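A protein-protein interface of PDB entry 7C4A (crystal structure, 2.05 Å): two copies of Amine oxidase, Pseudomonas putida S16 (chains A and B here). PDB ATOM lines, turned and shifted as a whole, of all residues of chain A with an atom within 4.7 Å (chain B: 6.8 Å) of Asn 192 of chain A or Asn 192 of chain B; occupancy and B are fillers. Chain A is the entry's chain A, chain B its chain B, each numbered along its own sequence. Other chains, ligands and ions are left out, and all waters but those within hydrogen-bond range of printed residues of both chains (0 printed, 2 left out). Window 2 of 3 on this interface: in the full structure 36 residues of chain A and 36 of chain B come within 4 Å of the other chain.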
ATOM      1  N   PHE A 186      29.117 -33.690  19.309  1.00  0.00           N
ATOM      2  CA  PHE A 186      27.728 -33.516  18.942  1.00  0.00           C
ATOM      3  C   PHE A 186      26.979 -32.787  20.081  1.00  0.00           C
ATOM      4  O   PHE A 186      26.226 -31.810  19.835  1.00  0.00           O
ATOM      5  CB  PHE A 186      27.131 -34.887  18.613  1.00  0.00           C
ATOM      6  CG  PHE A 186      25.680 -34.867  18.234  1.00  0.00           C
ATOM      7  CD1 PHE A 186      25.294 -34.689  16.914  1.00  0.00           C
ATOM      8  CD2 PHE A 186      24.700 -35.060  19.177  1.00  0.00           C
ATOM      9  CE1 PHE A 186      23.947 -34.680  16.562  1.00  0.00           C
ATOM     10  CE2 PHE A 186      23.353 -35.038  18.829  1.00  0.00           C
ATOM     11  CZ  PHE A 186      22.981 -34.850  17.521  1.00  0.00           C
ATOM     12  N   GLY A 189      27.526 -29.131  20.186  1.00  0.00           N
ATOM     13  CA  GLY A 189      26.755 -28.444  19.165  1.00  0.00           C
ATOM     14  C   GLY A 189      25.262 -28.440  19.418  1.00  0.00           C
ATOM     15  O   GLY A 189      24.477 -28.745  18.530  1.00  0.00           O
ATOM     16  N   GLY A 190      24.873 -28.133  20.661  1.00  0.00           N
ATOM     17  CA  GLY A 190      23.489 -28.057  21.055  1.00  0.00           C
ATOM     18  C   GLY A 190      22.695 -29.322  20.980  1.00  0.00           C
ATOM     19  O   GLY A 190      21.464 -29.282  20.842  1.00  0.00           O
ATOM     20  N   TRP A 191      23.396 -30.454  21.097  1.00  0.00           N
ATOM     21  CA  TRP A 191      22.795 -31.783  21.038  1.00  0.00           C
ATOM     22  C   TRP A 191      21.861 -31.957  19.834  1.00  0.00           C
ATOM     23  O   TRP A 191      20.853 -32.587  19.931  1.00  0.00           O
ATOM     24  CB  TRP A 191      22.000 -32.062  22.306  1.00  0.00           C
ATOM     25  CG  TRP A 191      22.752 -31.940  23.604  1.00  0.00           C
ATOM     26  CD1 TRP A 191      23.486 -32.927  24.237  1.00  0.00           C
ATOM     27  CD2 TRP A 191      22.780 -30.804  24.473  1.00  0.00           C
ATOM     28  NE1 TRP A 191      23.976 -32.454  25.437  1.00  0.00           N
ATOM     29  CE2 TRP A 191      23.538 -31.166  25.621  1.00  0.00           C
ATOM     30  CE3 TRP A 191      22.227 -29.517  24.404  1.00  0.00           C
ATOM     31  CZ2 TRP A 191      23.754 -30.293  26.685  1.00  0.00           C
ATOM     32  CZ3 TRP A 191      22.437 -28.632  25.488  1.00  0.00           C
ATOM     33  CH2 TRP A 191      23.214 -29.029  26.602  1.00  0.00           C
ATOM     34  N   ASN A 192      22.242 -31.386  18.690  1.00  0.00           N
ATOM     35  CA  ASN A 192      21.342 -31.269  17.576  1.00  0.00           C
ATOM     36  C   ASN A 192      22.119 -31.375  16.260  1.00  0.00           C
ATOM     37  O   ASN A 192      23.127 -30.694  16.055  1.00  0.00           O
ATOM     38  CB  ASN A 192      20.614 -29.927  17.735  1.00  0.00           C
ATOM     39  CG  ASN A 192      19.741 -29.618  16.591  1.00  0.00           C
ATOM     40  OD1 ASN A 192      20.174 -28.989  15.641  1.00  0.00           O
ATOM     41  ND2 ASN A 192      18.500 -30.090  16.641  1.00  0.00           N
ATOM     42  N   TYR A 193      21.658 -32.248  15.357  1.00  0.00           N
ATOM     43  CA  TYR A 193      22.358 -32.500  14.100  1.00  0.00           C
ATOM     44  C   TYR A 193      22.499 -31.243  13.245  1.00  0.00           C
ATOM     45  O   TYR A 193      23.578 -30.957  12.732  1.00  0.00           O
ATOM     46  CB  TYR A 193      21.582 -33.559  13.303  1.00  0.00           C
ATOM     47  CG  TYR A 193      22.126 -33.884  11.923  1.00  0.00           C
ATOM     48  CD1 TYR A 193      23.169 -34.789  11.763  1.00  0.00           C
ATOM     49  CD2 TYR A 193      21.568 -33.318  10.787  1.00  0.00           C
ATOM     50  CE1 TYR A 193      23.646 -35.123  10.508  1.00  0.00           C
ATOM     51  CE2 TYR A 193      22.015 -33.662   9.518  1.00  0.00           C
ATOM     52  CZ  TYR A 193      23.063 -34.566   9.382  1.00  0.00           C
ATOM     53  OH  TYR A 193      23.520 -34.902   8.121  1.00  0.00           O
ATOM     54  N   ASP A 194      21.417 -30.477  13.092  1.00  0.00           N
ATOM     55  CA  ASP A 194      21.459 -29.265  12.261  1.00  0.00           C
ATOM     56  C   ASP A 194      22.463 -28.258  12.781  1.00  0.00           C
ATOM     57  O   ASP A 194      23.257 -27.714  12.034  1.00  0.00           O
ATOM     58  CB  ASP A 194      20.065 -28.656  12.095  1.00  0.00           C
ATOM     59  CG  ASP A 194      19.201 -29.482  11.142  1.00  0.00           C
ATOM     60  OD1 ASP A 194      19.701 -30.036  10.151  1.00  0.00           O
ATOM     61  OD2 ASP A 194      18.033 -29.613  11.388  1.00  0.00           O
ATOM     62  N   ALA A 195      22.491 -28.068  14.096  1.00  0.00           N
ATOM     63  CA  ALA A 195      23.409 -27.095  14.691  1.00  0.00           C
ATOM     64  C   ALA A 195      24.840 -27.609  14.574  1.00  0.00           C
ATOM     65  O   ALA A 195      25.740 -26.900  14.142  1.00  0.00           O
ATOM     66  CB  ALA A 195      23.029 -26.816  16.147  1.00  0.00           C
ATOM     67  N   PHE A 196      25.058 -28.871  14.950  1.00  0.00           N
ATOM     68  CA  PHE A 196      26.375 -29.430  14.864  1.00  0.00           C
ATOM     69  C   PHE A 196      26.941 -29.374  13.442  1.00  0.00           C
ATOM     70  O   PHE A 196      28.098 -29.003  13.246  1.00  0.00           O
ATOM     71  CB  PHE A 196      26.408 -30.851  15.422  1.00  0.00           C
ATOM     72  CG  PHE A 196      27.756 -31.469  15.341  1.00  0.00           C
ATOM     73  CD1 PHE A 196      28.787 -31.000  16.157  1.00  0.00           C
ATOM     74  CD2 PHE A 196      28.028 -32.450  14.406  1.00  0.00           C
ATOM     75  CE1 PHE A 196      30.058 -31.525  16.084  1.00  0.00           C
ATOM     76  CE2 PHE A 196      29.310 -33.000  14.310  1.00  0.00           C
ATOM     77  CZ  PHE A 196      30.329 -32.531  15.153  1.00  0.00           C
ATOM     78  N   ARG B 111       5.981 -26.923  25.160  1.00  0.00           N
ATOM     79  CA  ARG B 111       6.840 -27.279  24.052  1.00  0.00           C
ATOM     80  C   ARG B 111       6.142 -27.094  22.685  1.00  0.00           C
ATOM     81  O   ARG B 111       6.693 -26.513  21.761  1.00  0.00           O
ATOM     82  CB  ARG B 111       7.333 -28.703  24.239  1.00  0.00           C
ATOM     83  CG  ARG B 111       8.140 -29.210  23.084  1.00  0.00           C
ATOM     84  CD  ARG B 111       8.549 -30.632  23.380  1.00  0.00           C
ATOM     85  NE  ARG B 111       9.724 -30.831  22.614  1.00  0.00           N
ATOM     86  CZ  ARG B 111      10.946 -31.039  23.079  1.00  0.00           C
ATOM     87  NH1 ARG B 111      11.216 -31.203  24.384  1.00  0.00           N
ATOM     88  NH2 ARG B 111      11.893 -31.143  22.165  1.00  0.00           N
ATOM     89  N   GLU B 115       7.602 -24.252  20.098  1.00  0.00           N
ATOM     90  CA  GLU B 115       8.097 -24.720  18.800  1.00  0.00           C
ATOM     91  C   GLU B 115       7.295 -24.149  17.648  1.00  0.00           C
ATOM     92  O   GLU B 115       7.876 -23.777  16.622  1.00  0.00           O
ATOM     93  CB  GLU B 115       8.192 -26.255  18.732  1.00  0.00           C
ATOM     94  CG  GLU B 115       9.307 -26.775  19.643  1.00  0.00           C
ATOM     95  CD  GLU B 115       9.645 -28.244  19.465  1.00  0.00           C
ATOM     96  OE1 GLU B 115       8.753 -29.076  19.199  1.00  0.00           O
ATOM     97  OE2 GLU B 115      10.845 -28.591  19.618  1.00  0.00           O
ATOM     98  N   TRP B 122      15.448 -20.893  12.017  1.00  0.00           N
ATOM     99  CA  TRP B 122      16.535 -21.231  11.091  1.00  0.00           C
ATOM    100  C   TRP B 122      16.573 -20.322   9.869  1.00  0.00           C
ATOM    101  O   TRP B 122      17.633 -19.855   9.469  1.00  0.00           O
ATOM    102  CB  TRP B 122      16.441 -22.669  10.613  1.00  0.00           C
ATOM    103  CG  TRP B 122      17.402 -23.572  11.277  1.00  0.00           C
ATOM    104  CD1 TRP B 122      17.112 -24.590  12.158  1.00  0.00           C
ATOM    105  CD2 TRP B 122      18.837 -23.544  11.147  1.00  0.00           C
ATOM    106  NE1 TRP B 122      18.289 -25.203  12.563  1.00  0.00           N
ATOM    107  CE2 TRP B 122      19.354 -24.570  11.968  1.00  0.00           C
ATOM    108  CE3 TRP B 122      19.730 -22.750  10.418  1.00  0.00           C
ATOM    109  CZ2 TRP B 122      20.722 -24.826  12.070  1.00  0.00           C
ATOM    110  CZ3 TRP B 122      21.088 -23.004  10.525  1.00  0.00           C
ATOM    111  CH2 TRP B 122      21.570 -24.041  11.344  1.00  0.00           C
ATOM    112  N   PHE B 186      16.186 -17.740  20.637  1.00  0.00           N
ATOM    113  CA  PHE B 186      15.990 -19.152  20.361  1.00  0.00           C
ATOM    114  C   PHE B 186      17.060 -19.636  19.372  1.00  0.00           C
ATOM    115  O   PHE B 186      17.705 -20.693  19.581  1.00  0.00           O
ATOM    116  CB  PHE B 186      14.557 -19.372  19.841  1.00  0.00           C
ATOM    117  CG  PHE B 186      14.228 -20.806  19.532  1.00  0.00           C
ATOM    118  CD1 PHE B 186      13.750 -21.658  20.510  1.00  0.00           C
ATOM    119  CD2 PHE B 186      14.365 -21.285  18.262  1.00  0.00           C
ATOM    120  CE1 PHE B 186      13.417 -22.982  20.206  1.00  0.00           C
ATOM    121  CE2 PHE B 186      14.042 -22.596  17.948  1.00  0.00           C
ATOM    122  CZ  PHE B 186      13.568 -23.444  18.923  1.00  0.00           C
ATOM    123  N   ALA B 187      17.282 -18.852  18.311  1.00  0.00           N
ATOM    124  CA  ALA B 187      18.337 -19.169  17.335  1.00  0.00           C
ATOM    125  C   ALA B 187      19.720 -19.267  17.991  1.00  0.00           C
ATOM    126  O   ALA B 187      20.478 -20.211  17.704  1.00  0.00           O
ATOM    127  CB  ALA B 187      18.320 -18.179  16.159  1.00  0.00           C
ATOM    128  N   GLY B 189      20.358 -20.279  20.848  1.00  0.00           N
ATOM    129  CA  GLY B 189      20.410 -21.549  21.585  1.00  0.00           C
ATOM    130  C   GLY B 189      20.355 -22.772  20.683  1.00  0.00           C
ATOM    131  O   GLY B 189      19.581 -23.700  20.923  1.00  0.00           O
ATOM    132  N   GLY B 190      21.143 -22.749  19.609  1.00  0.00           N
ATOM    133  CA  GLY B 190      21.245 -23.851  18.671  1.00  0.00           C
ATOM    134  C   GLY B 190      19.970 -24.182  17.904  1.00  0.00           C
ATOM    135  O   GLY B 190      19.783 -25.321  17.447  1.00  0.00           O
ATOM    136  N   TRP B 191      19.111 -23.169  17.731  1.00  0.00           N
ATOM    137  CA  TRP B 191      17.856 -23.297  17.039  1.00  0.00           C
ATOM    138  C   TRP B 191      17.024 -24.486  17.529  1.00  0.00           C
ATOM    139  O   TRP B 191      16.364 -25.139  16.760  1.00  0.00           O
ATOM    140  CB  TRP B 191      18.073 -23.452  15.540  1.00  0.00           C
ATOM    141  CG  TRP B 191      18.874 -22.369  14.859  1.00  0.00           C
ATOM    142  CD1 TRP B 191      18.392 -21.181  14.332  1.00  0.00           C
ATOM    143  CD2 TRP B 191      20.273 -22.392  14.570  1.00  0.00           C
ATOM    144  NE1 TRP B 191      19.407 -20.482  13.750  1.00  0.00           N
ATOM    145  CE2 TRP B 191      20.569 -21.200  13.857  1.00  0.00           C
ATOM    146  CE3 TRP B 191      21.301 -23.295  14.839  1.00  0.00           C
ATOM    147  CZ2 TRP B 191      21.862 -20.894  13.391  1.00  0.00           C
ATOM    148  CZ3 TRP B 191      22.596 -23.006  14.372  1.00  0.00           C
ATOM    149  CH2 TRP B 191      22.866 -21.798  13.670  1.00  0.00           C
ATOM    150  N   ASN B 192      17.051 -24.750  18.826  1.00  0.00           N
ATOM    151  CA  ASN B 192      16.524 -25.996  19.339  1.00  0.00           C
ATOM    152  C   ASN B 192      15.916 -25.762  20.740  1.00  0.00           C
ATOM    153  O   ASN B 192      16.550 -25.195  21.619  1.00  0.00           O
ATOM    154  CB  ASN B 192      17.704 -26.992  19.371  1.00  0.00           C
ATOM    155  CG  ASN B 192      17.336 -28.268  19.983  1.00  0.00           C
ATOM    156  OD1 ASN B 192      17.469 -28.459  21.195  1.00  0.00           O
ATOM    157  ND2 ASN B 192      16.801 -29.166  19.150  1.00  0.00           N
ATOM    158  N   TYR B 193      14.686 -26.223  20.942  1.00  0.00           N
ATOM    159  CA  TYR B 193      13.967 -26.016  22.196  1.00  0.00           C
ATOM    160  C   TYR B 193      14.707 -26.573  23.422  1.00  0.00           C
ATOM    161  O   TYR B 193      14.862 -25.899  24.428  1.00  0.00           O
ATOM    162  CB  TYR B 193      12.587 -26.661  22.093  1.00  0.00           C
ATOM    163  CG  TYR B 193      11.735 -26.574  23.347  1.00  0.00           C
ATOM    164  CD1 TYR B 193      11.002 -25.437  23.628  1.00  0.00           C
ATOM    165  CD2 TYR B 193      11.652 -27.659  24.235  1.00  0.00           C
ATOM    166  CE1 TYR B 193      10.210 -25.350  24.769  1.00  0.00           C
ATOM    167  CE2 TYR B 193      10.851 -27.603  25.366  1.00  0.00           C
ATOM    168  CZ  TYR B 193      10.126 -26.432  25.633  1.00  0.00           C
ATOM    169  OH  TYR B 193       9.321 -26.338  26.743  1.00  0.00           O
ATOM    170  N   ASP B 194      15.200 -27.801  23.328  1.00  0.00           N
ATOM    171  CA  ASP B 194      15.842 -28.442  24.476  1.00  0.00           C
ATOM    172  C   ASP B 194      17.107 -27.684  24.864  1.00  0.00           C
ATOM    173  O   ASP B 194      17.345 -27.405  26.039  1.00  0.00           O
ATOM    174  CB  ASP B 194      16.135 -29.909  24.191  1.00  0.00           C
ATOM    175  CG  ASP B 194      14.868 -30.751  24.166  1.00  0.00           C
ATOM    176  OD1 ASP B 194      13.985 -30.537  25.003  1.00  0.00           O
ATOM    177  OD2 ASP B 194      14.743 -31.578  23.304  1.00  0.00           O
ATOM    178  N   ALA B 195      17.893 -27.279  23.861  1.00  0.00           N
ATOM    179  CA  ALA B 195      19.130 -26.564  24.141  1.00  0.00           C
ATOM    180  C   ALA B 195      18.812 -25.179  24.709  1.00  0.00           C
ATOM    181  O   ALA B 195      19.338 -24.760  25.746  1.00  0.00           O
ATOM    182  CB  ALA B 195      19.984 -26.511  22.874  1.00  0.00           C
ATOM    183  N   PHE B 196      17.906 -24.459  24.047  1.00  0.00           N
ATOM    184  CA  PHE B 196      17.530 -23.151  24.525  1.00  0.00           C
ATOM    185  C   PHE B 196      16.992 -23.173  25.957  1.00  0.00           C
ATOM    186  O   PHE B 196      17.388 -22.344  26.784  1.00  0.00           O
ATOM    187  CB  PHE B 196      16.544 -22.484  23.571  1.00  0.00           C
ATOM    188  CG  PHE B 196      16.139 -21.129  24.023  1.00  0.00           C
ATOM    189  CD1 PHE B 196      17.053 -20.080  23.991  1.00  0.00           C
ATOM    190  CD2 PHE B 196      14.881 -20.911  24.548  1.00  0.00           C
ATOM    191  CE1 PHE B 196      16.707 -18.809  24.447  1.00  0.00           C
ATOM    192  CE2 PHE B 196      14.531 -19.646  25.017  1.00  0.00           C
ATOM    193  CZ  PHE B 196      15.449 -18.586  24.934  1.00  0.00           C
ATOM    194  N   MET B 197      16.092 -24.120  26.253  1.00  0.00           N
ATOM    195  CA  MET B 197      15.491 -24.218  27.581  1.00  0.00           C
ATOM    196  C   MET B 197      16.554 -24.494  28.656  1.00  0.00           C
ATOM    197  O   MET B 197      16.409 -24.044  29.803  1.00  0.00           O
ATOM    198  CB  MET B 197      14.398 -25.294  27.588  1.00  0.00           C
ATOM    199  CG  MET B 197      13.140 -24.884  26.827  1.00  0.00           C
ATOM    200  SD  MET B 197      12.279 -23.300  27.686  1.00  0.00           S
ATOM    201  CE  MET B 197      11.427 -23.950  29.362  1.00  0.00           C
ATOM    202  N   ASP B 198      17.625 -25.215  28.288  1.00  0.00           N
ATOM    203  CA  ASP B 198      18.710 -25.528  29.218  1.00  0.00           C
ATOM    204  C   ASP B 198      19.456 -24.275  29.681  1.00  0.00           C
ATOM    205  O   ASP B 198      20.114 -24.275  30.705  1.00  0.00           O
ATOM    206  CB  ASP B 198      19.689 -26.515  28.562  1.00  0.00           C
ATOM    207  CG  ASP B 198      20.460 -27.369  29.569  1.00  0.00           C
ATOM    208  OD1 ASP B 198      19.830 -27.898  30.507  1.00  0.00           O
ATOM    209  OD2 ASP B 198      21.709 -27.533  29.426  1.00  0.00           O
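Among the printed residues, merely in contact across the chains: Gly 190 of chain A with Ala 195 of chain B, Trp 191 of chain A with Asp 198 of chain B, Asp 194 of chain A with Trp 122 of chain B and Ala 195 of chain A with Gly 190 of chain B.
The side-chain amide oxygen (OD1) of Asn 192 of chain A is in hydrogen-bond range of the backbone NH (N) of Asp 194 of chain A (3.2 Å).
N of Ala 195 of chain A is in hydrogen-bond range of OD1 of Asn 192 of chain A (2.9 Å).
The backbone carbonyl oxygen (O) of Phe 186 of chain A is in hydrogen-bond range of the backbone NH (N) of Trp 191 of chain A (3.4 Å).
OD1 of Asn 192 of chain B sits at hydrogen-bond distance from N of Asp 194 of chain B (3.2 Å).
OD1 of Asn 192 of chain B is in hydrogen-bond range of N of Ala 195 of chain B.
Hydrophobic or aromatic side chains of chain B within 4 Å of the printed part of chain A: Trp 122 and Ala 195.
Along chain B the printed residues that touch a printed residue of chain A span positions 122 to 198.
Printed residues of chain A that touch a printed residue of chain B: Gly 190, Trp 191, Asn 192, Asp 194 and Ala 195.
Hydrophobic or aromatic side chains of chain A that line the printed part of chain B: Trp 191 and Ala 195.
Along chain A the printed residues that touch a printed residue of chain B span positions 190 to 195.
Among the printed residues, no Asp or Glu carboxylate lies within 4 Å of a Lys or Arg side-chain nitrogen of the other chain.
ND2 of Asn 192 of chain B sits close to ND2 of Asn 192 of chain A (3.2 Å).
Of the printed residues of chain B, Gly 190 of chain A touches Ala 195.
Of the printed residues of chain B, Trp 191 of chain A touches Asp 198.
Of the printed residues of chain B, Ala 195 of chain A touches Gly 190.
Of the printed residues of chain A, Trp 122 of chain B touches Asp 194.
Of chain A, only Asn 192 comes within 4 Å of Asn 192 of chain B.
Printed residues of chain A within 4 Å of Ala 195 of chain B: Gly 190.
The nearest residue of chain A that does not touch Asn 192 of chain B is Gly 190 of chain A (4.1 Å).
The nearest printed residue of chain A that does not touch Gly 190 of chain B is Asn 192 of chain A (4.1 Å).
Gly 190 of chain A touches Ala 195 of chain B, and with the chains exchanged Ala 195 of chain A touches Gly 190 of chain B.
Asn 192 of chain B touches its own counterpart, Asn 192 of chain A.
Of the 5 pairs that touch across the chains among the printed residues, 3 have their exchanged pair printed and touching as well.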
